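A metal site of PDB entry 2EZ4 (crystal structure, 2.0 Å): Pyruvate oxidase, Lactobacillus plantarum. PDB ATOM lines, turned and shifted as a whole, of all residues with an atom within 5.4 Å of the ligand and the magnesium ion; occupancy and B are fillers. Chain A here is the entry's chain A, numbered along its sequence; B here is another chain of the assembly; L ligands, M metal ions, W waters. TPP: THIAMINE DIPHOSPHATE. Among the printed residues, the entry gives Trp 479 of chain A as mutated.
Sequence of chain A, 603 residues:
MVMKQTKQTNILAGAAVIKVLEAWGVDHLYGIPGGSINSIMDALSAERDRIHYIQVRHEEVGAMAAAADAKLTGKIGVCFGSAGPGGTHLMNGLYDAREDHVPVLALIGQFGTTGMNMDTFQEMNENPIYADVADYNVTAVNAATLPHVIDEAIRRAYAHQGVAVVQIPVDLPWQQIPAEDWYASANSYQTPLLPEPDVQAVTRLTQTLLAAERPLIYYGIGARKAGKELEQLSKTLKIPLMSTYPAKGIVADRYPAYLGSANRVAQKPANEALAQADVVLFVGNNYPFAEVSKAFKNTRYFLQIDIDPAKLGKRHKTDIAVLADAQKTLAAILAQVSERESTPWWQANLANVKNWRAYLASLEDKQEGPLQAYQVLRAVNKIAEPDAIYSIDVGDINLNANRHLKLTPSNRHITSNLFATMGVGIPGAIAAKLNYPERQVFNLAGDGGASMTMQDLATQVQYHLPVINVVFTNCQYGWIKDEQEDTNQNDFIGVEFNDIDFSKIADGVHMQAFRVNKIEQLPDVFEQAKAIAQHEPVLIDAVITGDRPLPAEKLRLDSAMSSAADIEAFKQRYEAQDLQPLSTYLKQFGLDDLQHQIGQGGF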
ATOM      1  N   ASN A  92     -30.507  13.245  22.303  1.00  0.00           N
ATOM      2  CA  ASN A  92     -29.873  12.223  21.463  1.00  0.00           C
ATOM      3  C   ASN A  92     -30.021  10.818  22.006  1.00  0.00           C
ATOM      4  O   ASN A  92     -30.182   9.874  21.217  1.00  0.00           O
ATOM      5  CB  ASN A  92     -28.408  12.540  21.130  1.00  0.00           C
ATOM      6  CG  ASN A  92     -28.283  13.537  19.975  1.00  0.00           C
ATOM      7  OD1 ASN A  92     -28.906  14.600  19.995  1.00  0.00           O
ATOM      8  ND2 ASN A  92     -27.481  13.204  18.975  1.00  0.00           N
ATOM      9  N   ASP A 393     -19.334   2.714  19.110  1.00  0.00           N
ATOM     10  CA  ASP A 393     -19.772   4.025  18.671  1.00  0.00           C
ATOM     11  C   ASP A 393     -20.221   3.958  17.192  1.00  0.00           C
ATOM     12  O   ASP A 393     -20.597   2.896  16.705  1.00  0.00           O
ATOM     13  CB  ASP A 393     -18.674   5.055  18.886  1.00  0.00           C
ATOM     14  CG  ASP A 393     -19.204   6.419  19.252  1.00  0.00           C
ATOM     15  OD1 ASP A 393     -19.619   7.170  18.327  1.00  0.00           O
ATOM     16  OD2 ASP A 393     -19.176   6.759  20.454  1.00  0.00           O
ATOM     17  N   VAL A 394     -20.248   5.105  16.510  1.00  0.00           N
ATOM     18  CA  VAL A 394     -20.810   5.196  15.161  1.00  0.00           C
ATOM     19  C   VAL A 394     -19.767   5.717  14.176  1.00  0.00           C
ATOM     20  O   VAL A 394     -19.150   6.753  14.407  1.00  0.00           O
ATOM     21  CB  VAL A 394     -22.090   6.099  15.179  1.00  0.00           C
ATOM     22  CG1 VAL A 394     -22.563   6.444  13.777  1.00  0.00           C
ATOM     23  CG2 VAL A 394     -23.193   5.403  15.973  1.00  0.00           C
ATOM     24  N   GLY A 395     -19.609   5.023  13.050  1.00  0.00           N
ATOM     25  CA  GLY A 395     -18.623   5.400  12.035  1.00  0.00           C
ATOM     26  C   GLY A 395     -17.957   4.145  11.463  1.00  0.00           C
ATOM     27  O   GLY A 395     -18.542   3.074  11.498  1.00  0.00           O
ATOM     28  N   ASP A 396     -16.723   4.284  10.965  1.00  0.00           N
ATOM     29  CA  ASP A 396     -15.968   3.131  10.445  1.00  0.00           C
ATOM     30  C   ASP A 396     -15.935   1.954  11.409  1.00  0.00           C
ATOM     31  O   ASP A 396     -15.892   0.813  10.961  1.00  0.00           O
ATOM     32  CB  ASP A 396     -14.508   3.498  10.115  1.00  0.00           C
ATOM     33  CG  ASP A 396     -14.341   4.073   8.727  1.00  0.00           C
ATOM     34  OD1 ASP A 396     -15.303   4.134   7.945  1.00  0.00           O
ATOM     35  OD2 ASP A 396     -13.192   4.488   8.412  1.00  0.00           O
ATOM     36  N   ILE A 397     -15.926   2.234  12.703  1.00  0.00           N
ATOM     37  CA  ILE A 397     -15.878   1.185  13.734  1.00  0.00           C
ATOM     38  C   ILE A 397     -17.024   0.171  13.631  1.00  0.00           C
ATOM     39  O   ILE A 397     -16.803  -1.011  13.875  1.00  0.00           O
ATOM     40  CB  ILE A 397     -15.775   1.752  15.205  1.00  0.00           C
ATOM     41  CG1 ILE A 397     -15.467   0.611  16.204  1.00  0.00           C
ATOM     42  CG2 ILE A 397     -17.073   2.503  15.634  1.00  0.00           C
ATOM     43  CD1 ILE A 397     -14.120  -0.125  15.991  1.00  0.00           C
ATOM     44  N   PHE A 419     -31.065   5.371  14.829  1.00  0.00           N
ATOM     45  CA  PHE A 419     -30.796   6.815  14.989  1.00  0.00           C
ATOM     46  C   PHE A 419     -29.319   7.063  14.748  1.00  0.00           C
ATOM     47  O   PHE A 419     -28.938   8.102  14.215  1.00  0.00           O
ATOM     48  CB  PHE A 419     -31.175   7.291  16.405  1.00  0.00           C
ATOM     49  CG  PHE A 419     -31.261   8.817  16.561  1.00  0.00           C
ATOM     50  CD1 PHE A 419     -32.119   9.572  15.745  1.00  0.00           C
ATOM     51  CD2 PHE A 419     -30.540   9.465  17.563  1.00  0.00           C
ATOM     52  CE1 PHE A 419     -32.231  10.985  15.918  1.00  0.00           C
ATOM     53  CE2 PHE A 419     -30.624  10.866  17.748  1.00  0.00           C
ATOM     54  CZ  PHE A 419     -31.496  11.621  16.905  1.00  0.00           C
ATOM     55  N   ALA A 420     -28.490   6.089  15.121  1.00  0.00           N
ATOM     56  CA  ALA A 420     -27.068   6.129  14.817  1.00  0.00           C
ATOM     57  C   ALA A 420     -26.414   7.423  15.315  1.00  0.00           C
ATOM     58  O   ALA A 420     -25.687   8.089  14.557  1.00  0.00           O
ATOM     59  CB  ALA A 420     -26.827   5.944  13.278  1.00  0.00           C
ATOM     60  N   THR A 421     -26.699   7.786  16.569  1.00  0.00           N
ATOM     61  CA  THR A 421     -26.007   8.895  17.211  1.00  0.00           C
ATOM     62  C   THR A 421     -24.584   8.507  17.586  1.00  0.00           C
ATOM     63  O   THR A 421     -24.362   7.498  18.284  1.00  0.00           O
ATOM     64  CB  THR A 421     -26.772   9.475  18.437  1.00  0.00           C
ATOM     65  OG1 THR A 421     -26.077  10.624  18.924  1.00  0.00           O
ATOM     66  CG2 THR A 421     -26.967   8.432  19.606  1.00  0.00           C
ATOM     67  N   MET A 422     -23.631   9.308  17.125  1.00  0.00           N
ATOM     68  CA  MET A 422     -22.255   9.254  17.596  1.00  0.00           C
ATOM     69  C   MET A 422     -22.227   9.601  19.079  1.00  0.00           C
ATOM     70  O   MET A 422     -23.153  10.240  19.593  1.00  0.00           O
ATOM     71  CB  MET A 422     -21.392  10.261  16.836  1.00  0.00           C
ATOM     72  CG  MET A 422     -21.071   9.880  15.398  1.00  0.00           C
ATOM     73  SD  MET A 422     -20.431  11.329  14.537  1.00  0.00           S
ATOM     74  CE  MET A 422     -18.806  11.488  15.284  1.00  0.00           C
ATOM     75  N   ALA A 445     -14.584   3.083  19.729  1.00  0.00           N
ATOM     76  CA  ALA A 445     -15.075   4.327  19.189  1.00  0.00           C
ATOM     77  C   ALA A 445     -14.041   5.007  18.296  1.00  0.00           C
ATOM     78  O   ALA A 445     -12.830   4.937  18.563  1.00  0.00           O
ATOM     79  CB  ALA A 445     -15.475   5.269  20.340  1.00  0.00           C
ATOM     80  N   GLY A 446     -14.517   5.659  17.252  1.00  0.00           N
ATOM     81  CA  GLY A 446     -13.662   6.558  16.485  1.00  0.00           C
ATOM     82  C   GLY A 446     -13.388   7.828  17.277  1.00  0.00           C
ATOM     83  O   GLY A 446     -14.037   8.092  18.303  1.00  0.00           O
ATOM     84  N   ASP A 447     -12.413   8.604  16.800  1.00  0.00           N
ATOM     85  CA  ASP A 447     -12.040   9.846  17.439  1.00  0.00           C
ATOM     86  C   ASP A 447     -13.135  10.906  17.399  1.00  0.00           C
ATOM     87  O   ASP A 447     -13.304  11.641  18.343  1.00  0.00           O
ATOM     88  CB  ASP A 447     -10.694  10.414  16.939  1.00  0.00           C
ATOM     89  CG  ASP A 447     -10.559  10.490  15.421  1.00  0.00           C
ATOM     90  OD1 ASP A 447     -11.487  10.160  14.647  1.00  0.00           O
ATOM     91  OD2 ASP A 447      -9.455  10.885  14.990  1.00  0.00           O
ATOM     92  N   GLY A 448     -13.889  10.973  16.299  1.00  0.00           N
ATOM     93  CA  GLY A 448     -15.012  11.903  16.202  1.00  0.00           C
ATOM     94  C   GLY A 448     -16.060  11.602  17.242  1.00  0.00           C
ATOM     95  O   GLY A 448     -16.499  12.489  17.966  1.00  0.00           O
ATOM     96  N   GLY A 449     -16.491  10.337  17.331  1.00  0.00           N
ATOM     97  CA  GLY A 449     -17.537   9.946  18.295  1.00  0.00           C
ATOM     98  C   GLY A 449     -17.088  10.030  19.741  1.00  0.00           C
ATOM     99  O   GLY A 449     -17.808  10.522  20.601  1.00  0.00           O
ATOM    100  N   ALA A 450     -15.886   9.542  20.012  1.00  0.00           N
ATOM    101  CA  ALA A 450     -15.270   9.651  21.345  1.00  0.00           C
ATOM    102  C   ALA A 450     -15.125  11.102  21.820  1.00  0.00           C
ATOM    103  O   ALA A 450     -15.335  11.395  23.002  1.00  0.00           O
ATOM    104  CB  ALA A 450     -13.922   8.919  21.367  1.00  0.00           C
ATOM    105  N   MET A 452     -17.173  13.550  21.153  1.00  0.00           N
ATOM    106  CA  MET A 452     -18.476  14.124  21.534  1.00  0.00           C
ATOM    107  C   MET A 452     -18.877  13.856  22.972  1.00  0.00           C
ATOM    108  O   MET A 452     -19.571  14.679  23.576  1.00  0.00           O
ATOM    109  CB  MET A 452     -19.575  13.615  20.597  1.00  0.00           C
ATOM    110  CG  MET A 452     -19.476  14.242  19.211  1.00  0.00           C
ATOM    111  SD  MET A 452     -20.748  13.647  18.111  1.00  0.00           S
ATOM    112  CE  MET A 452     -20.351  14.630  16.629  1.00  0.00           C
ATOM    113  N   PHE A 472     -10.070   4.965  18.018  1.00  0.00           N
ATOM    114  CA  PHE A 472      -9.485   4.827  16.688  1.00  0.00           C
ATOM    115  C   PHE A 472      -9.267   6.205  16.105  1.00  0.00           C
ATOM    116  O   PHE A 472     -10.193   6.839  15.586  1.00  0.00           O
ATOM    117  CB  PHE A 472     -10.396   3.989  15.787  1.00  0.00           C
ATOM    118  CG  PHE A 472     -10.509   2.538  16.223  1.00  0.00           C
ATOM    119  CD1 PHE A 472     -11.262   2.192  17.350  1.00  0.00           C
ATOM    120  CD2 PHE A 472      -9.839   1.542  15.529  1.00  0.00           C
ATOM    121  CE1 PHE A 472     -11.360   0.855  17.766  1.00  0.00           C
ATOM    122  CE2 PHE A 472      -9.954   0.188  15.928  1.00  0.00           C
ATOM    123  CZ  PHE A 472     -10.705  -0.149  17.051  1.00  0.00           C
ATOM    124  N   ASN A 474      -7.985   8.548  13.544  1.00  0.00           N
ATOM    125  CA  ASN A 474      -7.543   8.761  12.171  1.00  0.00           C
ATOM    126  C   ASN A 474      -7.523  10.238  11.784  1.00  0.00           C
ATOM    127  O   ASN A 474      -7.196  10.566  10.652  1.00  0.00           O
ATOM    128  CB  ASN A 474      -8.388   7.924  11.177  1.00  0.00           C
ATOM    129  CG  ASN A 474      -9.876   8.128  11.342  1.00  0.00           C
ATOM    130  OD1 ASN A 474     -10.310   8.981  12.112  1.00  0.00           O
ATOM    131  ND2 ASN A 474     -10.662   7.379  10.591  1.00  0.00           N
ATOM    132  N   CYS A 475      -7.878  11.115  12.735  1.00  0.00           N
ATOM    133  CA  CYS A 475      -7.982  12.563  12.494  1.00  0.00           C
ATOM    134  C   CYS A 475      -8.962  12.859  11.351  1.00  0.00           C
ATOM    135  O   CYS A 475      -8.766  13.824  10.587  1.00  0.00           O
ATOM    136  CB  CYS A 475      -6.594  13.170  12.206  1.00  0.00           C
ATOM    137  SG  CYS A 475      -5.462  13.039  13.625  1.00  0.00           S
ATOM    138  N   GLN A 476     -10.001  12.037  11.259  1.00  0.00           N
ATOM    139  CA  GLN A 476     -11.012  12.175  10.218  1.00  0.00           C
ATOM    140  C   GLN A 476     -12.354  11.770  10.761  1.00  0.00           C
ATOM    141  O   GLN A 476     -12.435  11.053  11.765  1.00  0.00           O
ATOM    142  CB  GLN A 476     -10.710  11.249   9.013  1.00  0.00           C
ATOM    143  CG  GLN A 476      -9.339  11.447   8.365  1.00  0.00           C
ATOM    144  CD  GLN A 476      -9.037  10.429   7.288  1.00  0.00           C
ATOM    145  OE1 GLN A 476      -8.189  10.658   6.430  1.00  0.00           O
ATOM    146  NE2 GLN A 476      -9.733   9.294   7.327  1.00  0.00           N
ATOM    147  N   TYR A 477     -13.406  12.225  10.100  1.00  0.00           N
ATOM    148  CA  TYR A 477     -14.680  11.552  10.131  1.00  0.00           C
ATOM    149  C   TYR A 477     -14.603  10.641   8.919  1.00  0.00           C
ATOM    150  O   TYR A 477     -15.106  10.998   7.836  1.00  0.00           O
ATOM    151  CB  TYR A 477     -15.853  12.565   9.973  1.00  0.00           C
ATOM    152  CG  TYR A 477     -16.014  13.536  11.132  1.00  0.00           C
ATOM    153  CD1 TYR A 477     -16.153  13.081  12.452  1.00  0.00           C
ATOM    154  CD2 TYR A 477     -16.023  14.921  10.902  1.00  0.00           C
ATOM    155  CE1 TYR A 477     -16.299  13.992  13.531  1.00  0.00           C
ATOM    156  CE2 TYR A 477     -16.164  15.830  11.960  1.00  0.00           C
ATOM    157  CZ  TYR A 477     -16.301  15.356  13.268  1.00  0.00           C
ATOM    158  OH  TYR A 477     -16.435  16.258  14.296  1.00  0.00           O
ATOM    159  N   GLY A 478     -13.953   9.473   9.076  1.00  0.00           N
ATOM    160  CA  GLY A 478     -13.633   8.608   7.945  1.00  0.00           C
ATOM    161  C   GLY A 478     -14.885   8.144   7.211  1.00  0.00           C
ATOM    162  O   GLY A 478     -14.946   8.189   5.993  1.00  0.00           O
ATOM    163  N   TRP A 479     -15.892   7.711   7.971  1.00  0.00           N
ATOM    164  CA  TRP A 479     -17.187   7.288   7.416  1.00  0.00           C
ATOM    165  C   TRP A 479     -17.720   8.299   6.403  1.00  0.00           C
ATOM    166  O   TRP A 479     -18.222   7.908   5.325  1.00  0.00           O
ATOM    167  CB  TRP A 479     -18.189   7.091   8.556  1.00  0.00           C
ATOM    168  CG  TRP A 479     -19.441   6.287   8.219  1.00  0.00           C
ATOM    169  CD1 TRP A 479     -20.722   6.752   8.124  1.00  0.00           C
ATOM    170  CD2 TRP A 479     -19.509   4.868   7.978  1.00  0.00           C
ATOM    171  NE1 TRP A 479     -21.592   5.717   7.829  1.00  0.00           N
ATOM    172  CE2 TRP A 479     -20.868   4.545   7.742  1.00  0.00           C
ATOM    173  CE3 TRP A 479     -18.555   3.840   7.933  1.00  0.00           C
ATOM    174  CZ2 TRP A 479     -21.300   3.239   7.464  1.00  0.00           C
ATOM    175  CZ3 TRP A 479     -18.989   2.525   7.660  1.00  0.00           C
ATOM    176  CH2 TRP A 479     -20.355   2.253   7.427  1.00  0.00           C
ATOM    177  N   ILE A 480     -17.617   9.590   6.742  1.00  0.00           N
ATOM    178  CA  ILE A 480     -18.147  10.673   5.899  1.00  0.00           C
ATOM    179  C   ILE A 480     -17.175  11.096   4.793  1.00  0.00           C
ATOM    180  O   ILE A 480     -17.599  11.470   3.693  1.00  0.00           O
ATOM    181  CB  ILE A 480     -18.534  11.922   6.747  1.00  0.00           C
ATOM    182  CG1 ILE A 480     -19.389  11.511   7.965  1.00  0.00           C
ATOM    183  CG2 ILE A 480     -19.253  12.997   5.871  1.00  0.00           C
ATOM    184  CD1 ILE A 480     -20.599  10.693   7.621  1.00  0.00           C
ATOM    185  N   PHE A 497      -9.438  16.639  10.264  1.00  0.00           N
ATOM    186  CA  PHE A 497      -9.271  17.615  11.320  1.00  0.00           C
ATOM    187  C   PHE A 497      -8.033  17.361  12.169  1.00  0.00           C
ATOM    188  O   PHE A 497      -7.301  16.389  11.961  1.00  0.00           O
ATOM    189  CB  PHE A 497     -10.541  17.679  12.186  1.00  0.00           C
ATOM    190  CG  PHE A 497     -11.048  16.331  12.656  1.00  0.00           C
ATOM    191  CD1 PHE A 497     -10.350  15.586  13.611  1.00  0.00           C
ATOM    192  CD2 PHE A 497     -12.248  15.814  12.142  1.00  0.00           C
ATOM    193  CE1 PHE A 497     -10.830  14.346  14.056  1.00  0.00           C
ATOM    194  CE2 PHE A 497     -12.738  14.575  12.585  1.00  0.00           C
ATOM    195  CZ  PHE A 497     -12.034  13.843  13.522  1.00  0.00           C
ATOM    196  N   ILE B  32     -21.166  19.929  11.426  1.00  0.00           N
ATOM    197  CA  ILE B  32     -20.470  18.672  11.218  1.00  0.00           C
ATOM    198  C   ILE B  32     -21.165  18.008  10.031  1.00  0.00           C
ATOM    199  O   ILE B  32     -22.414  17.967   9.989  1.00  0.00           O
ATOM    200  CB  ILE B  32     -20.544  17.748  12.482  1.00  0.00           C
ATOM    201  CG1 ILE B  32     -19.792  18.396  13.644  1.00  0.00           C
ATOM    202  CG2 ILE B  32     -20.052  16.295  12.150  1.00  0.00           C
ATOM    203  CD1 ILE B  32     -19.812  17.626  14.955  1.00  0.00           C
ATOM    204  N   PRO B  33     -20.381  17.538   9.051  1.00  0.00           N
ATOM    205  CA  PRO B  33     -20.963  16.976   7.823  1.00  0.00           C
ATOM    206  C   PRO B  33     -21.544  15.602   8.091  1.00  0.00           C
ATOM    207  O   PRO B  33     -21.292  15.019   9.142  1.00  0.00           O
ATOM    208  CB  PRO B  33     -19.769  16.870   6.872  1.00  0.00           C
ATOM    209  CG  PRO B  33     -18.586  16.686   7.798  1.00  0.00           C
ATOM    210  CD  PRO B  33     -18.892  17.504   9.020  1.00  0.00           C
ATOM    211  N   GLY B  34     -22.335  15.113   7.133  1.00  0.00           N
ATOM    212  CA  GLY B  34     -22.867  13.753   7.177  1.00  0.00           C
ATOM    213  C   GLY B  34     -23.402  13.480   5.795  1.00  0.00           C
ATOM    214  O   GLY B  34     -23.620  14.421   5.020  1.00  0.00           O
ATOM    215  N   GLU B  59     -22.156  19.230  17.539  1.00  0.00           N
ATOM    216  CA  GLU B  59     -23.080  20.172  16.881  1.00  0.00           C
ATOM    217  C   GLU B  59     -23.701  21.210  17.797  1.00  0.00           C
ATOM    218  O   GLU B  59     -24.089  22.275  17.316  1.00  0.00           O
ATOM    219  CB  GLU B  59     -24.166  19.469  16.065  1.00  0.00           C
ATOM    220  CG  GLU B  59     -23.634  18.631  14.925  1.00  0.00           C
ATOM    221  CD  GLU B  59     -23.346  17.185  15.332  1.00  0.00           C
ATOM    222  OE1 GLU B  59     -23.236  16.897  16.555  1.00  0.00           O
ATOM    223  OE2 GLU B  59     -23.229  16.318  14.423  1.00  0.00           O
ATOM    224  N   SER B  82     -26.382  17.192  10.482  1.00  0.00           N
ATOM    225  CA  SER B  82     -26.872  16.104   9.630  1.00  0.00           C
ATOM    226  C   SER B  82     -28.182  15.480  10.171  1.00  0.00           C
ATOM    227  O   SER B  82     -28.593  15.743  11.318  1.00  0.00           O
ATOM    228  CB  SER B  82     -25.789  15.030   9.474  1.00  0.00           C
ATOM    229  OG  SER B  82     -25.365  14.607  10.759  1.00  0.00           O
ATOM    230  N   PRO B  85     -29.387  12.601  14.586  1.00  0.00           N
ATOM    231  CA  PRO B  85     -28.583  13.044  15.717  1.00  0.00           C
ATOM    232  C   PRO B  85     -27.759  14.315  15.515  1.00  0.00           C
ATOM    233  O   PRO B  85     -27.445  14.991  16.498  1.00  0.00           O
ATOM    234  CB  PRO B  85     -27.652  11.856  15.981  1.00  0.00           C
ATOM    235  CG  PRO B  85     -27.591  11.119  14.695  1.00  0.00           C
ATOM    236  CD  PRO B  85     -28.952  11.276  14.081  1.00  0.00           C
ATOM    237  N   GLY B  86     -27.395  14.633  14.276  1.00  0.00           N
ATOM    238  CA  GLY B  86     -26.656  15.868  13.995  1.00  0.00           C
ATOM    239  C   GLY B  86     -27.532  17.066  14.356  1.00  0.00           C
ATOM    240  O   GLY B  86     -27.127  17.950  15.100  1.00  0.00           O
ATOM    241  N   HIS B  89     -28.567  17.379  18.140  1.00  0.00           N
ATOM    242  CA  HIS B  89     -27.459  17.938  18.942  1.00  0.00           C
ATOM    243  C   HIS B  89     -27.483  19.479  18.983  1.00  0.00           C
ATOM    244  O   HIS B  89     -26.929  20.095  19.898  1.00  0.00           O
ATOM    245  CB  HIS B  89     -26.099  17.454  18.411  1.00  0.00           C
ATOM    246  CG  HIS B  89     -25.519  16.293  19.156  1.00  0.00           C
ATOM    247  ND1 HIS B  89     -24.354  15.666  18.767  1.00  0.00           N
ATOM    248  CD2 HIS B  89     -25.916  15.666  20.290  1.00  0.00           C
ATOM    249  CE1 HIS B  89     -24.076  14.695  19.619  1.00  0.00           C
ATOM    250  NE2 HIS B  89     -25.007  14.669  20.551  1.00  0.00           N
ATOM    251  N   GLN B 122     -31.492   6.146   9.603  1.00  0.00           N
ATOM    252  CA  GLN B 122     -31.443   7.495  10.169  1.00  0.00           C
ATOM    253  C   GLN B 122     -32.480   8.437   9.547  1.00  0.00           C
ATOM    254  O   GLN B 122     -32.280   9.661   9.495  1.00  0.00           O
ATOM    255  CB  GLN B 122     -30.034   8.047   9.979  1.00  0.00           C
ATOM    256  CG  GLN B 122     -29.527   8.893  11.076  1.00  0.00           C
ATOM    257  CD  GLN B 122     -28.062   9.162  10.928  1.00  0.00           C
ATOM    258  OE1 GLN B 122     -27.574   9.439   9.835  1.00  0.00           O
ATOM    259  NE2 GLN B 122     -27.332   9.080  12.032  1.00  0.00           N
HETATM  260  N1' TPP L   1     -23.407  13.774  14.240  1.00  0.00           N
HETATM  261  C2' TPP L   1     -23.941  12.851  15.123  1.00  0.00           C
HETATM  262  CM2 TPP L   1     -24.249  13.221  16.547  1.00  0.00           C
HETATM  263  N3' TPP L   1     -24.190  11.546  14.739  1.00  0.00           N
HETATM  264  C4' TPP L   1     -23.932  11.135  13.449  1.00  0.00           C
HETATM  265  N4' TPP L   1     -24.233   9.875  13.122  1.00  0.00           N
HETATM  266  C5' TPP L   1     -23.400  12.052  12.534  1.00  0.00           C
HETATM  267  C6' TPP L   1     -23.133  13.373  12.935  1.00  0.00           C
HETATM  268  C7' TPP L   1     -23.069  11.607  11.112  1.00  0.00           C
HETATM  269  N3  TPP L   1     -21.891  10.731  11.140  1.00  0.00           N
HETATM  270  C2  TPP L   1     -21.907   9.332  11.063  1.00  0.00           C
HETATM  271  S1  TPP L   1     -20.447   8.599  11.133  1.00  0.00           S
HETATM  272  C5  TPP L   1     -19.720  10.051  11.252  1.00  0.00           C
HETATM  273  C4  TPP L   1     -20.593  11.148  11.247  1.00  0.00           C
HETATM  274  CM4 TPP L   1     -20.114  12.579  11.351  1.00  0.00           C
HETATM  275  C6  TPP L   1     -18.204  10.074  11.335  1.00  0.00           C
HETATM  276  C7  TPP L   1     -17.644   9.326  12.537  1.00  0.00           C
HETATM  277  O7  TPP L   1     -16.293   9.750  12.722  1.00  0.00           O
HETATM  278  PA  TPP L   1     -15.365   8.944  13.726  1.00  0.00           P
HETATM  279  O1A TPP L   1     -14.025   9.627  13.846  1.00  0.00           O
HETATM  280  O2A TPP L   1     -16.057   8.740  15.029  1.00  0.00           O
HETATM  281  O3A TPP L   1     -15.200   7.485  13.057  1.00  0.00           O
HETATM  282  PB  TPP L   1     -14.299   7.073  11.769  1.00  0.00           P
HETATM  283  O1B TPP L   1     -15.232   6.817  10.603  1.00  0.00           O
HETATM  284  O2B TPP L   1     -13.626   5.819  12.245  1.00  0.00           O
HETATM  285  O3B TPP L   1     -13.282   8.140  11.433  1.00  0.00           O
HETATM  286 MG    MG M   1     -12.296   9.266  12.981  1.00  0.00          MG
HETATM  287  O   HOH W   1     -26.551  12.222  11.033  1.00  0.00           O
HETATM  288  O   HOH W   2     -15.424   4.745  14.091  1.00  0.00           O
HETATM  289  O   HOH W   3     -25.034   8.821  10.341  1.00  0.00           O
HETATM  290  O   HOH W   4     -12.031   7.210  13.816  1.00  0.00           O
HETATM  291  O   HOH W   5     -11.652   3.864  12.298  1.00  0.00           O
HETATM  292  O   HOH W   6     -16.946   6.496  15.849  1.00  0.00           O
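O1A of the ligand binds the magnesium ion, 2.0 Å away. OD1 of Asp 447 binds the magnesium ion (2.1 Å). An oxygen (O3B) of the ligand is bound to the magnesium ion, 2.2 Å away. O of Gln 476 binds the magnesium ion. The magnesium ion is bound by the side-chain amide oxygen (OD1) of Asn 474, at 2.2 Å. The magnesium ion is bound by water W4 (2.2 Å). The magnesium ion has six donor atoms within binding distance.
Residues that only touch the ligand: His 89 of chain B, Tyr 477, Ser 82 of chain B, Pro 85 of chain B, Pro 33 of chain B, Ile 480, Val 394, Gly 446, Gly 395, Ile 32 of chain B, Met 452, Gly 86 of chain B and Thr 421. Hydrophobic or aromatic side chains that line the ligand: Val 394, Met 422, Met 452, Tyr 477, Trp 479, Ile 480, Ile 32 of chain B, Pro 85 of chain B and His 89 of chain B. Of the 35 residues printed, 25 come within 4 Å of the ligand. The nearest printed residue that does not touch the ligand is Asn 92 (4.04 Å).
Three residues have an atom within 4 Å of the magnesium ion: Asp 447, Asn 474 and Gln 476. The nearest printed residue that does not touch the magnesium ion is Gly 448 (4.1 Å).
A nitrogen (N1') of the ligand lies within hydrogen-bond range of the side-chain carboxylate (OE2) of Glu 59 of chain B (2.6 Å). O of Ala 420 lies within hydrogen-bond range of N4' of the ligand (2.7 Å). N of Gly 478 is in hydrogen-bond range of O1B of the ligand, at 3.3 Å. O2A of the ligand sits at hydrogen-bond distance from N of Gly 448 (3.4 Å). The backbone NH of Gly 449 is in hydrogen-bond range of an oxygen (O2A) of the ligand (2.8 Å). N of Trp 479 is in hydrogen-bond range of O1B of the ligand, at 2.9 Å. An oxygen (O1B) of the ligand sits at hydrogen-bond distance from the backbone NH of Asp 396 (3.0 Å). N of Met 422 lies within hydrogen-bond range of N3' of the ligand, 3.3 Å away. A nitrogen (N4') of the ligand sits close to the side-chain amide nitrogen (NE2) of Gln 122 of chain B (3.4 Å).
Water W4 lies within hydrogen-bond range of the backbone carbonyl oxygen of Phe 472, an oxygen (O2B) of the ligand and the backbone NH of Asp 447. Water W6 lies within hydrogen-bond range of O2A of the ligand (2.5 Å), O of Val 394 (2.6 Å) and N of Gly 446 (2.9 Å). Water W3 lies within hydrogen-bond range of OE1 of Gln 122 of chain B and N4' of the ligand. Water W1 lies within hydrogen-bond range of OG of Ser 82 of chain B (2.7 Å) and OE1 of Gln 122 of chain B (3.2 Å).
O of Phe 472 lies within hydrogen-bond range of N of Asp 447 (3.1 Å). The side-chain carboxylate of Asp 447 is in hydrogen-bond range of the backbone NH of Cys 475, 2.8 Å away. The side-chain carboxylate (OE1) of Glu 59 of chain B sits at hydrogen-bond distance from a ring nitrogen (ND1) of His 89 of chain B. O of Ala 420 sits at hydrogen-bond distance from NE2 of Gln 122 of chain B (3.2 Å). The side-chain amide nitrogen of Asn 92 lies close to a ring nitrogen (NE2) of His 89 of chain B (3.3 Å). O of Phe 419 lies within hydrogen-bond range of NE2 of Gln 122 of chain B, at 2.9 Å. ND2 of Asn 92 is in hydrogen-bond range of O of Pro 85 of chain B, at 3.1 Å. The side-chain hydroxyl (OG1) of Thr 421 lies within hydrogen-bond range of the side-chain amide nitrogen (ND2) of Asn 92, 2.9 Å away.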
